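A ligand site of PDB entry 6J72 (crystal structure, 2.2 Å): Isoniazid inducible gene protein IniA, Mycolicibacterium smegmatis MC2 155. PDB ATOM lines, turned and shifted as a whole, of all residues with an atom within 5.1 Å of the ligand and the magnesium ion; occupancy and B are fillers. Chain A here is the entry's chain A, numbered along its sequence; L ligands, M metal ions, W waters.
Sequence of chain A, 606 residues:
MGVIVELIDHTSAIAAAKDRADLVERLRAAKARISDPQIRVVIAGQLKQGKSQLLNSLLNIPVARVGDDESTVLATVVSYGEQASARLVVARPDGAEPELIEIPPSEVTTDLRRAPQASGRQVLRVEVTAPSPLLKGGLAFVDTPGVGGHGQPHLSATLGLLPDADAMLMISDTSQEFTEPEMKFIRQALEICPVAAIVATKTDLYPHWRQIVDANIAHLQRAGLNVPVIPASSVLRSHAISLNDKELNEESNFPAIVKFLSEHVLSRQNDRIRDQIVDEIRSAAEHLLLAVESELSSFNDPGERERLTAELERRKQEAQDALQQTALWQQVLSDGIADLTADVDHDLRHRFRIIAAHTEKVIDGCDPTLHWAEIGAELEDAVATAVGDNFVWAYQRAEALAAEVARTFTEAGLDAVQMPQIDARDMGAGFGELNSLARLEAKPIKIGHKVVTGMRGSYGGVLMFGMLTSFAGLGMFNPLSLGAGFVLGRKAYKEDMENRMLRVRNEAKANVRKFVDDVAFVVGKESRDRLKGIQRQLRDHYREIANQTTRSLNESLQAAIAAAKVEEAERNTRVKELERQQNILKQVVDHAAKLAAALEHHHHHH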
ATOM      1  N   GLN A  46       9.865 -21.765  11.183  1.00  0.00           N
ATOM      2  CA  GLN A  46       8.496 -22.006  11.646  1.00  0.00           C
ATOM      3  C   GLN A  46       8.030 -20.860  12.544  1.00  0.00           C
ATOM      4  O   GLN A  46       8.793 -19.938  12.817  1.00  0.00           O
ATOM      5  CB  GLN A  46       8.411 -23.343  12.383  1.00  0.00           C
ATOM      6  CG  GLN A  46       8.986 -24.514  11.584  1.00  0.00           C
ATOM      7  CD  GLN A  46       8.281 -25.830  11.884  1.00  0.00           C
ATOM      8  OE1 GLN A  46       7.267 -26.158  11.276  1.00  0.00           O
ATOM      9  NE2 GLN A  46       8.834 -26.592  12.824  1.00  0.00           N
ATOM     10  N   LEU A  47       6.792 -20.898  12.960  1.00  0.00           N
ATOM     11  CA  LEU A  47       6.239 -19.825  13.782  1.00  0.00           C
ATOM     12  C   LEU A  47       6.904 -19.594  15.134  1.00  0.00           C
ATOM     13  O   LEU A  47       7.387 -20.496  15.751  1.00  0.00           O
ATOM     14  CB  LEU A  47       4.738 -19.940  13.949  1.00  0.00           C
ATOM     15  CG  LEU A  47       3.954 -21.182  14.308  1.00  0.00           C
ATOM     16  CD1 LEU A  47       4.709 -22.385  14.766  1.00  0.00           C
ATOM     17  CD2 LEU A  47       2.769 -20.914  15.180  1.00  0.00           C
ATOM     18  N   LYS A  48       6.935 -18.347  15.549  1.00  0.00           N
ATOM     19  CA  LYS A  48       7.382 -17.957  16.880  1.00  0.00           C
ATOM     20  C   LYS A  48       8.847 -18.300  17.183  1.00  0.00           C
ATOM     21  O   LYS A  48       9.230 -18.396  18.350  1.00  0.00           O
ATOM     22  CB  LYS A  48       6.488 -18.619  17.930  1.00  0.00           C
ATOM     23  CG  LYS A  48       5.035 -18.196  17.845  1.00  0.00           C
ATOM     24  CD  LYS A  48       4.906 -16.685  17.961  1.00  0.00           C
ATOM     25  CE  LYS A  48       3.609 -16.187  17.342  1.00  0.00           C
ATOM     26  NZ  LYS A  48       3.700 -14.755  16.948  1.00  0.00           N
ATOM     27  N   GLN A  49       9.657 -18.451  16.149  1.00  0.00           N
ATOM     28  CA  GLN A  49      11.067 -18.793  16.349  1.00  0.00           C
ATOM     29  C   GLN A  49      11.915 -17.551  16.610  1.00  0.00           C
ATOM     30  O   GLN A  49      13.074 -17.659  17.026  1.00  0.00           O
ATOM     31  CB  GLN A  49      11.610 -19.561  15.144  1.00  0.00           C
ATOM     32  CG  GLN A  49      11.004 -20.946  14.978  1.00  0.00           C
ATOM     33  CD  GLN A  49      11.042 -21.756  16.264  1.00  0.00           C
ATOM     34  OE1 GLN A  49      12.114 -22.122  16.741  1.00  0.00           O
ATOM     35  NE2 GLN A  49       9.877 -22.033  16.824  1.00  0.00           N
ATOM     36  N   GLY A  50      11.332 -16.371  16.380  1.00  0.00           N
ATOM     37  CA  GLY A  50      12.016 -15.124  16.660  1.00  0.00           C
ATOM     38  C   GLY A  50      12.502 -14.431  15.404  1.00  0.00           C
ATOM     39  O   GLY A  50      13.481 -13.678  15.429  1.00  0.00           O
ATOM     40  N   LYS A  51      11.813 -14.686  14.293  1.00  0.00           N
ATOM     41  CA  LYS A  51      12.198 -14.125  12.998  1.00  0.00           C
ATOM     42  C   LYS A  51      12.066 -12.611  12.962  1.00  0.00           C
ATOM     43  O   LYS A  51      13.017 -11.904  12.632  1.00  0.00           O
ATOM     44  CB  LYS A  51      11.360 -14.757  11.884  1.00  0.00           C
ATOM     45  CG  LYS A  51      11.492 -16.266  11.781  1.00  0.00           C
ATOM     46  CD  LYS A  51      10.764 -16.801  10.560  1.00  0.00           C
ATOM     47  CE  LYS A  51       9.267 -16.546  10.643  1.00  0.00           C
ATOM     48  NZ  LYS A  51       8.668 -17.162  11.857  1.00  0.00           N
ATOM     49  N   SER A  52      10.882 -12.123  13.316  1.00  0.00           N
ATOM     50  CA  SER A  52      10.597 -10.695  13.280  1.00  0.00           C
ATOM     51  C   SER A  52      11.441  -9.906  14.273  1.00  0.00           C
ATOM     52  O   SER A  52      11.956  -8.831  13.949  1.00  0.00           O
ATOM     53  CB  SER A  52       9.105 -10.452  13.552  1.00  0.00           C
ATOM     54  OG  SER A  52       8.318 -10.965  12.506  1.00  0.00           O
ATOM     55  N   GLN A  53      11.581 -10.427  15.485  1.00  0.00           N
ATOM     56  CA  GLN A  53      12.383  -9.782  16.519  1.00  0.00           C
ATOM     57  C   GLN A  53      13.836  -9.673  16.080  1.00  0.00           C
ATOM     58  O   GLN A  53      14.500  -8.669  16.366  1.00  0.00           O
ATOM     59  CB  GLN A  53      12.278 -10.545  17.837  1.00  0.00           C
ATOM     60  CG  GLN A  53      13.007  -9.882  18.991  1.00  0.00           C
ATOM     61  CD  GLN A  53      12.495  -8.475  19.262  1.00  0.00           C
ATOM     62  OE1 GLN A  53      13.140  -7.489  18.897  1.00  0.00           O
ATOM     63  NE2 GLN A  53      11.340  -8.385  19.905  1.00  0.00           N
ATOM     64  N   LEU A  54      14.324 -10.697  15.396  1.00  0.00           N
ATOM     65  CA  LEU A  54      15.681 -10.692  14.863  1.00  0.00           C
ATOM     66  C   LEU A  54      15.877  -9.534  13.898  1.00  0.00           C
ATOM     67  O   LEU A  54      16.864  -8.797  13.974  1.00  0.00           O
ATOM     68  CB  LEU A  54      16.003 -12.015  14.167  1.00  0.00           C
ATOM     69  CG  LEU A  54      17.426 -12.145  13.612  1.00  0.00           C
ATOM     70  CD1 LEU A  54      18.343 -12.786  14.643  1.00  0.00           C
ATOM     71  CD2 LEU A  54      17.445 -12.919  12.306  1.00  0.00           C
ATOM     72  N   ARG A  65       6.501  -7.017  12.962  1.00  0.00           N
ATOM     73  CA  ARG A  65       5.497  -7.046  14.006  1.00  0.00           C
ATOM     74  C   ARG A  65       5.763  -8.199  14.942  1.00  0.00           C
ATOM     75  O   ARG A  65       5.839  -9.326  14.499  1.00  0.00           O
ATOM     76  CB  ARG A  65       4.125  -7.269  13.409  1.00  0.00           C
ATOM     77  CG  ARG A  65       4.104  -7.988  12.080  1.00  0.00           C
ATOM     78  CD  ARG A  65       2.767  -7.748  11.386  1.00  0.00           C
ATOM     79  NE  ARG A  65       1.643  -7.996  12.284  1.00  0.00           N
ATOM     80  CZ  ARG A  65       0.372  -7.958  11.915  1.00  0.00           C
ATOM     81  NH1 ARG A  65      -0.595  -8.182  12.780  1.00  0.00           N
ATOM     82  NH2 ARG A  65       0.056  -7.677  10.676  1.00  0.00           N
ATOM     83  N   VAL A  66       5.891  -7.964  16.232  1.00  0.00           N
ATOM     84  CA  VAL A  66       6.154  -9.100  17.109  1.00  0.00           C
ATOM     85  C   VAL A  66       5.181  -9.202  18.274  1.00  0.00           C
ATOM     86  O   VAL A  66       5.121  -8.329  19.116  1.00  0.00           O
ATOM     87  CB  VAL A  66       7.646  -9.224  17.537  1.00  0.00           C
ATOM     88  CG1 VAL A  66       8.555  -8.414  16.627  1.00  0.00           C
ATOM     89  CG2 VAL A  66       7.917  -8.917  19.005  1.00  0.00           C
ATOM     90  N   GLY A  67       4.497 -10.335  18.323  1.00  0.00           N
ATOM     91  CA  GLY A  67       3.490 -10.608  19.325  1.00  0.00           C
ATOM     92  C   GLY A  67       3.576 -12.052  19.719  1.00  0.00           C
ATOM     93  O   GLY A  67       4.079 -12.866  18.966  1.00  0.00           O
ATOM     94  N   ASP A  68       3.007 -12.386  20.863  1.00  0.00           N
ATOM     95  CA  ASP A  68       3.096 -13.734  21.389  1.00  0.00           C
ATOM     96  C   ASP A  68       2.125 -14.713  20.747  1.00  0.00           C
ATOM     97  O   ASP A  68       2.294 -15.919  20.835  1.00  0.00           O
ATOM     98  CB  ASP A  68       2.889 -13.716  22.894  1.00  0.00           C
ATOM     99  CG  ASP A  68       3.912 -14.500  23.600  1.00  0.00           C
ATOM    100  OD1 ASP A  68       4.885 -13.900  24.061  1.00  0.00           O
ATOM    101  OD2 ASP A  68       3.739 -15.720  23.694  1.00  0.00           O
ATOM    102  N   GLU A  70       0.349 -13.923  17.037  1.00  0.00           N
ATOM    103  CA  GLU A  70      -0.203 -13.219  15.910  1.00  0.00           C
ATOM    104  C   GLU A  70       0.954 -12.837  14.987  1.00  0.00           C
ATOM    105  O   GLU A  70       1.614 -13.679  14.408  1.00  0.00           O
ATOM    106  CB  GLU A  70      -1.072 -12.012  16.350  1.00  0.00           C
ATOM    107  CG  GLU A  70      -0.680 -11.396  17.687  1.00  0.00           C
ATOM    108  CD  GLU A  70      -0.362  -9.919  17.591  1.00  0.00           C
ATOM    109  OE1 GLU A  70      -0.214  -9.289  18.645  1.00  0.00           O
ATOM    110  OE2 GLU A  70      -0.274  -9.392  16.468  1.00  0.00           O
ATOM    111  N   SER A  71       1.162 -11.544  14.858  1.00  0.00           N
ATOM    112  CA  SER A  71       2.262 -11.009  14.137  1.00  0.00           C
ATOM    113  C   SER A  71       2.287 -11.336  12.668  1.00  0.00           C
ATOM    114  O   SER A  71       1.376 -10.962  11.997  1.00  0.00           O
ATOM    115  CB  SER A  71       3.510 -11.407  14.856  1.00  0.00           C
ATOM    116  OG  SER A  71       3.307 -11.012  16.197  1.00  0.00           O
ATOM    117  N   THR A  72       3.336 -11.935  12.151  1.00  0.00           N
ATOM    118  CA  THR A  72       3.534 -11.902  10.711  1.00  0.00           C
ATOM    119  C   THR A  72       2.601 -12.792   9.908  1.00  0.00           C
ATOM    120  O   THR A  72       2.582 -13.975  10.070  1.00  0.00           O
ATOM    121  CB  THR A  72       4.979 -12.222  10.375  1.00  0.00           C
ATOM    122  OG1 THR A  72       5.823 -11.704  11.385  1.00  0.00           O
ATOM    123  CG2 THR A  72       5.351 -11.601   9.108  1.00  0.00           C
ATOM    124  N   ASP A 143      10.941 -10.727   5.765  1.00  0.00           N
ATOM    125  CA  ASP A 143      10.302 -11.370   6.896  1.00  0.00           C
ATOM    126  C   ASP A 143       9.193 -12.278   6.372  1.00  0.00           C
ATOM    127  O   ASP A 143       8.468 -11.915   5.450  1.00  0.00           O
ATOM    128  CB  ASP A 143       9.742 -10.332   7.875  1.00  0.00           C
ATOM    129  CG  ASP A 143       9.497 -10.905   9.253  1.00  0.00           C
ATOM    130  OD1 ASP A 143       9.908 -12.051   9.509  1.00  0.00           O
ATOM    131  OD2 ASP A 143       8.894 -10.188  10.096  1.00  0.00           O
ATOM    132  N   THR A 144       9.083 -13.473   6.945  1.00  0.00           N
ATOM    133  CA  THR A 144       8.124 -14.454   6.462  1.00  0.00           C
ATOM    134  C   THR A 144       6.986 -14.680   7.457  1.00  0.00           C
ATOM    135  O   THR A 144       7.183 -14.542   8.670  1.00  0.00           O
ATOM    136  CB  THR A 144       8.807 -15.805   6.166  1.00  0.00           C
ATOM    137  OG1 THR A 144       9.391 -16.332   7.361  1.00  0.00           O
ATOM    138  CG2 THR A 144       9.891 -15.627   5.114  1.00  0.00           C
ATOM    139  N   PRO A 145       5.788 -15.002   6.962  1.00  0.00           N
ATOM    140  CA  PRO A 145       4.643 -15.213   7.849  1.00  0.00           C
ATOM    141  C   PRO A 145       4.763 -16.475   8.697  1.00  0.00           C
ATOM    142  O   PRO A 145       5.597 -17.327   8.418  1.00  0.00           O
ATOM    143  CB  PRO A 145       3.462 -15.331   6.868  1.00  0.00           C
ATOM    144  CG  PRO A 145       4.075 -15.812   5.605  1.00  0.00           C
ATOM    145  CD  PRO A 145       5.421 -15.145   5.544  1.00  0.00           C
ATOM    146  N   GLY A 146       3.938 -16.567   9.729  1.00  0.00           N
ATOM    147  CA  GLY A 146       3.922 -17.731  10.591  1.00  0.00           C
ATOM    148  C   GLY A 146       3.487 -18.972   9.832  1.00  0.00           C
ATOM    149  O   GLY A 146       2.405 -19.005   9.237  1.00  0.00           O
ATOM    150  N   VAL A 147       4.344 -19.992   9.843  1.00  0.00           N
ATOM    151  CA  VAL A 147       4.030 -21.266   9.201  1.00  0.00           C
ATOM    152  C   VAL A 147       4.349 -22.414  10.146  1.00  0.00           C
ATOM    153  O   VAL A 147       5.146 -22.256  11.074  1.00  0.00           O
ATOM    154  CB  VAL A 147       4.823 -21.450   7.888  1.00  0.00           C
ATOM    155  CG1 VAL A 147       4.327 -20.496   6.811  1.00  0.00           C
ATOM    156  CG2 VAL A 147       6.317 -21.249   8.127  1.00  0.00           C
ATOM    157  N   LYS A 202      17.261 -16.878  20.721  1.00  0.00           N
ATOM    158  CA  LYS A 202      16.796 -16.940  22.106  1.00  0.00           C
ATOM    159  C   LYS A 202      17.778 -17.628  23.058  1.00  0.00           C
ATOM    160  O   LYS A 202      17.366 -18.358  23.962  1.00  0.00           O
ATOM    161  CB  LYS A 202      15.433 -17.628  22.180  1.00  0.00           C
ATOM    162  CG  LYS A 202      14.366 -16.996  21.305  1.00  0.00           C
ATOM    163  CD  LYS A 202      13.023 -17.688  21.483  1.00  0.00           C
ATOM    164  CE  LYS A 202      12.013 -17.206  20.464  1.00  0.00           C
ATOM    165  NZ  LYS A 202      10.761 -18.016  20.497  1.00  0.00           N
ATOM    166  N   ASP A 204      19.452 -16.185  25.253  1.00  0.00           N
ATOM    167  CA  ASP A 204      19.280 -15.537  26.547  1.00  0.00           C
ATOM    168  C   ASP A 204      18.188 -16.209  27.363  1.00  0.00           C
ATOM    169  O   ASP A 204      18.121 -16.046  28.582  1.00  0.00           O
ATOM    170  CB  ASP A 204      18.951 -14.059  26.359  1.00  0.00           C
ATOM    171  CG  ASP A 204      17.605 -13.849  25.705  1.00  0.00           C
ATOM    172  OD1 ASP A 204      17.524 -13.917  24.458  1.00  0.00           O
ATOM    173  OD2 ASP A 204      16.613 -13.608  26.436  1.00  0.00           O
ATOM    174  N   LEU A 205      17.331 -16.965  26.700  1.00  0.00           N
ATOM    175  CA  LEU A 205      16.172 -17.570  27.339  1.00  0.00           C
ATOM    176  C   LEU A 205      16.415 -19.018  27.744  1.00  0.00           C
ATOM    177  O   LEU A 205      15.847 -19.509  28.723  1.00  0.00           O
ATOM    178  CB  LEU A 205      14.953 -17.488  26.420  1.00  0.00           C
ATOM    179  CG  LEU A 205      13.611 -17.942  27.000  1.00  0.00           C
ATOM    180  CD1 LEU A 205      13.212 -17.071  28.176  1.00  0.00           C
ATOM    181  CD2 LEU A 205      12.529 -17.943  25.928  1.00  0.00           C
ATOM    182  N   SER A 233      21.060 -13.693  20.338  1.00  0.00           N
ATOM    183  CA  SER A 233      19.981 -13.225  21.208  1.00  0.00           C
ATOM    184  C   SER A 233      19.579 -11.813  20.800  1.00  0.00           C
ATOM    185  O   SER A 233      20.315 -10.854  21.035  1.00  0.00           O
ATOM    186  CB  SER A 233      20.412 -13.254  22.672  1.00  0.00           C
ATOM    187  OG  SER A 233      19.438 -12.635  23.491  1.00  0.00           O
ATOM    188  N   SER A 234      18.406 -11.694  20.189  1.00  0.00           N
ATOM    189  CA  SER A 234      17.895 -10.406  19.738  1.00  0.00           C
ATOM    190  C   SER A 234      17.669  -9.476  20.925  1.00  0.00           C
ATOM    191  O   SER A 234      17.834  -8.256  20.826  1.00  0.00           O
ATOM    192  CB  SER A 234      16.589 -10.588  18.960  1.00  0.00           C
ATOM    193  OG  SER A 234      16.792 -11.427  17.832  1.00  0.00           O
ATOM    194  N   VAL A 235      17.287 -10.073  22.046  1.00  0.00           N
ATOM    195  CA  VAL A 235      17.054  -9.373  23.294  1.00  0.00           C
ATOM    196  C   VAL A 235      18.316  -8.673  23.800  1.00  0.00           C
ATOM    197  O   VAL A 235      18.296  -7.475  24.114  1.00  0.00           O
ATOM    198  CB  VAL A 235      16.491 -10.354  24.348  1.00  0.00           C
ATOM    199  CG1 VAL A 235      16.681  -9.836  25.749  1.00  0.00           C
ATOM    200  CG2 VAL A 235      15.016 -10.604  24.085  1.00  0.00           C
HETATM  201  P1  LIG L   1       5.718 -15.305  13.692  1.00  0.00           P
HETATM  202  O1  LIG L   1       5.857 -14.045  12.881  1.00  0.00           O
HETATM  203  O2  LIG L   1       4.299 -15.438  14.197  1.00  0.00           O
HETATM  204  O3  LIG L   1       6.077 -16.499  12.846  1.00  0.00           O
HETATM  205  O4  LIG L   1       6.721 -15.233  14.962  1.00  0.00           O
HETATM  206  P2  LIG L   1       8.278 -14.863  14.764  1.00  0.00           P
HETATM  207  O5  LIG L   1       8.405 -13.584  13.970  1.00  0.00           O
HETATM  208  O6  LIG L   1       9.032 -15.990  14.107  1.00  0.00           O
HETATM  209  O7  LIG L   1       8.836 -14.607  16.251  1.00  0.00           O
HETATM  210  P3  LIG L   1       8.758 -13.149  16.943  1.00  0.00           P
HETATM  211  O8  LIG L   1       9.968 -12.338  16.549  1.00  0.00           O
HETATM  212  O9  LIG L   1       7.483 -12.436  16.597  1.00  0.00           O
HETATM  213  O10 LIG L   1       8.804 -13.484  18.510  1.00  0.00           O
HETATM  214  C1  LIG L   1       8.354 -14.716  19.032  1.00  0.00           C
HETATM  215  C2  LIG L   1       8.275 -14.553  20.546  1.00  0.00           C
HETATM  216  O11 LIG L   1       9.557 -14.876  21.055  1.00  0.00           O
HETATM  217  C3  LIG L   1       7.991 -13.108  20.918  1.00  0.00           C
HETATM  218  O12 LIG L   1       6.962 -13.063  21.891  1.00  0.00           O
HETATM  219  C4  LIG L   1       9.268 -12.583  21.534  1.00  0.00           C
HETATM  220  O13 LIG L   1       9.006 -11.858  22.707  1.00  0.00           O
HETATM  221  C5  LIG L   1      10.093 -13.826  21.824  1.00  0.00           C
HETATM  222  N1  LIG L   1      11.495 -13.609  21.427  1.00  0.00           N
HETATM  223  C6  LIG L   1      11.960 -13.321  20.173  1.00  0.00           C
HETATM  224  N2  LIG L   1      13.314 -13.212  20.234  1.00  0.00           N
HETATM  225  C7  LIG L   1      13.707 -13.433  21.509  1.00  0.00           C
HETATM  226  C8  LIG L   1      14.951 -13.455  22.117  1.00  0.00           C
HETATM  227  O14 LIG L   1      15.970 -13.227  21.459  1.00  0.00           O
HETATM  228  N3  LIG L   1      15.045 -13.723  23.470  1.00  0.00           N
HETATM  229  C9  LIG L   1      13.901 -13.970  24.206  1.00  0.00           C
HETATM  230  N4  LIG L   1      13.981 -14.233  25.503  1.00  0.00           N
HETATM  231  N5  LIG L   1      12.664 -13.959  23.589  1.00  0.00           N
HETATM  232  C10 LIG L   1      12.576 -13.688  22.263  1.00  0.00           C
HETATM  233 MG    MG M   1       7.124 -12.561  12.604  1.00  0.00          MG
HETATM  234  O   HOH W   1      15.004 -13.306  17.886  1.00  0.00           O
HETATM  235  O   HOH W   2       8.084 -13.499  10.852  1.00  0.00           O
HETATM  236  O   HOH W   3      17.037 -14.086  19.412  1.00  0.00           O
HETATM  237  O   HOH W   4       2.489 -17.007  13.732  1.00  0.00           O
HETATM  238  O   HOH W   5       6.258 -11.653  14.341  1.00  0.00           O
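N of Lys 48 lies within hydrogen-bond range of O4 of the ligand (3.2 Å). O12 of the ligand sits at hydrogen-bond distance from OD1 of Asp 68 (3.1 Å). O7 of the ligand is in hydrogen-bond range of N of Gly 50 (3.1 Å). An oxygen (O6) of the ligand lies within hydrogen-bond range of the backbone NH (N) of Gln 49, at 3.3 Å. NZ of Lys 51 lies within salt-bridge range of O6 of the ligand, 2.6 Å away. A nitrogen (N3) of the ligand sits at hydrogen-bond distance from the side-chain carboxylate (OD1) of Asp 204 (2.7 Å). An oxygen (O6) of the ligand lies within hydrogen-bond range of the backbone NH (N) of Lys 51. The backbone NH (N) of Ser 234 lies within hydrogen-bond range of an oxygen (O14) of the ligand (3.1 Å). The side-chain amino group (NZ) of Lys 48 lies within salt-bridge range of an oxygen (O2) of the ligand, 2.9 Å away. The backbone NH (N) of Gln 53 is in hydrogen-bond range of an oxygen (O8) of the ligand, at 2.7 Å. An oxygen (O11) of the ligand lies within hydrogen-bond range of the side-chain amino group of Lys 202 (3.4 Å). O14 of the ligand lies within hydrogen-bond range of N of Val 235 (3.5 Å). The backbone NH (N) of Ser 52 is in hydrogen-bond range of an oxygen (O8) of the ligand (3.4 Å). An oxygen (O1) of the ligand lies close to the backbone NH of Thr 72, at 3.4 Å.
O of Lys 48 lies within hydrogen-bond range of NZ of Lys 202 (2.7 Å). NZ of Lys 48 lies within hydrogen-bond range of O of Glu 70 (3.5 Å). The backbone carbonyl oxygen (O) of Ser 71 sits at hydrogen-bond distance from the guanidinium group (NE) of Arg 65 (3.0 Å). The backbone carbonyl oxygen of Thr 72 is in hydrogen-bond range of the backbone NH of Gly 146, 2.9 Å away. The side-chain amino group of Lys 51 lies within hydrogen-bond range of the backbone carbonyl oxygen of Gln 46 (2.9 Å). The side-chain carboxylate (OD1) of Asp 204 lies within hydrogen-bond range of the side-chain hydroxyl (OG) of Ser 233, 2.5 Å away. The side-chain carboxylate (OE2) of Glu 70 is in salt-bridge range of the guanidinium group (NH1) of Arg 65, 3.9 Å away. The side-chain carboxylate of Asp 143 lies close to the side-chain hydroxyl of Ser 52 (2.6 Å).
An oxygen (O2) of the ligand lies close to the backbone carbonyl oxygen (O) of Glu 70 (3.2 Å). Leu 47 touches the ligand (CA to O3, 3.5 Å). CB of Val 66 touches O9 of the ligand, at 3.4 Å. CA of Gly 146 touches O3 of the ligand, 3.4 Å away. CB of Leu 205 touches N4 of the ligand, 3.5 Å away. Ser 233 touches the ligand (C to O14, 3.9 Å). Of the 27 residues printed, 18 come within 4 Å of the ligand.
Residues that only touch the magnesium ion: Arg 65 and Asp 143. Of the 27 residues printed, 4 come within 4 Å of the magnesium ion. The nearest printed residue that does not touch the magnesium ion is Thr 144 (4.4 Å).
The magnesium ion is bound by an oxygen (O1) of the ligand (2.0 Å), the side-chain hydroxyl (OG1) of Thr 72 (2.0 Å), the side-chain hydroxyl (OG) of Ser 52 (2.0 Å), an oxygen (O5) of the ligand (2.1 Å), water W5 (2.1 Å) and water W2 (2.2 Å).
Water W2 lies within hydrogen-bond range of the backbone carbonyl oxygen (O) of Thr 144 (2.6 Å) and the side-chain carboxylate (OD1) of Asp 143 (2.7 Å). Water W3 lies within hydrogen-bond range of an oxygen (O14) of the ligand (2.5 Å), the backbone NH (N) of Ser 234 (2.9 Å) and the backbone NH (N) of Lys 202 (3.1 Å). Water W1 lies within hydrogen-bond range of the side-chain hydroxyl (OG) of Ser 234, a nitrogen (N2) of the ligand and the backbone carbonyl oxygen (O) of Gly 50.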
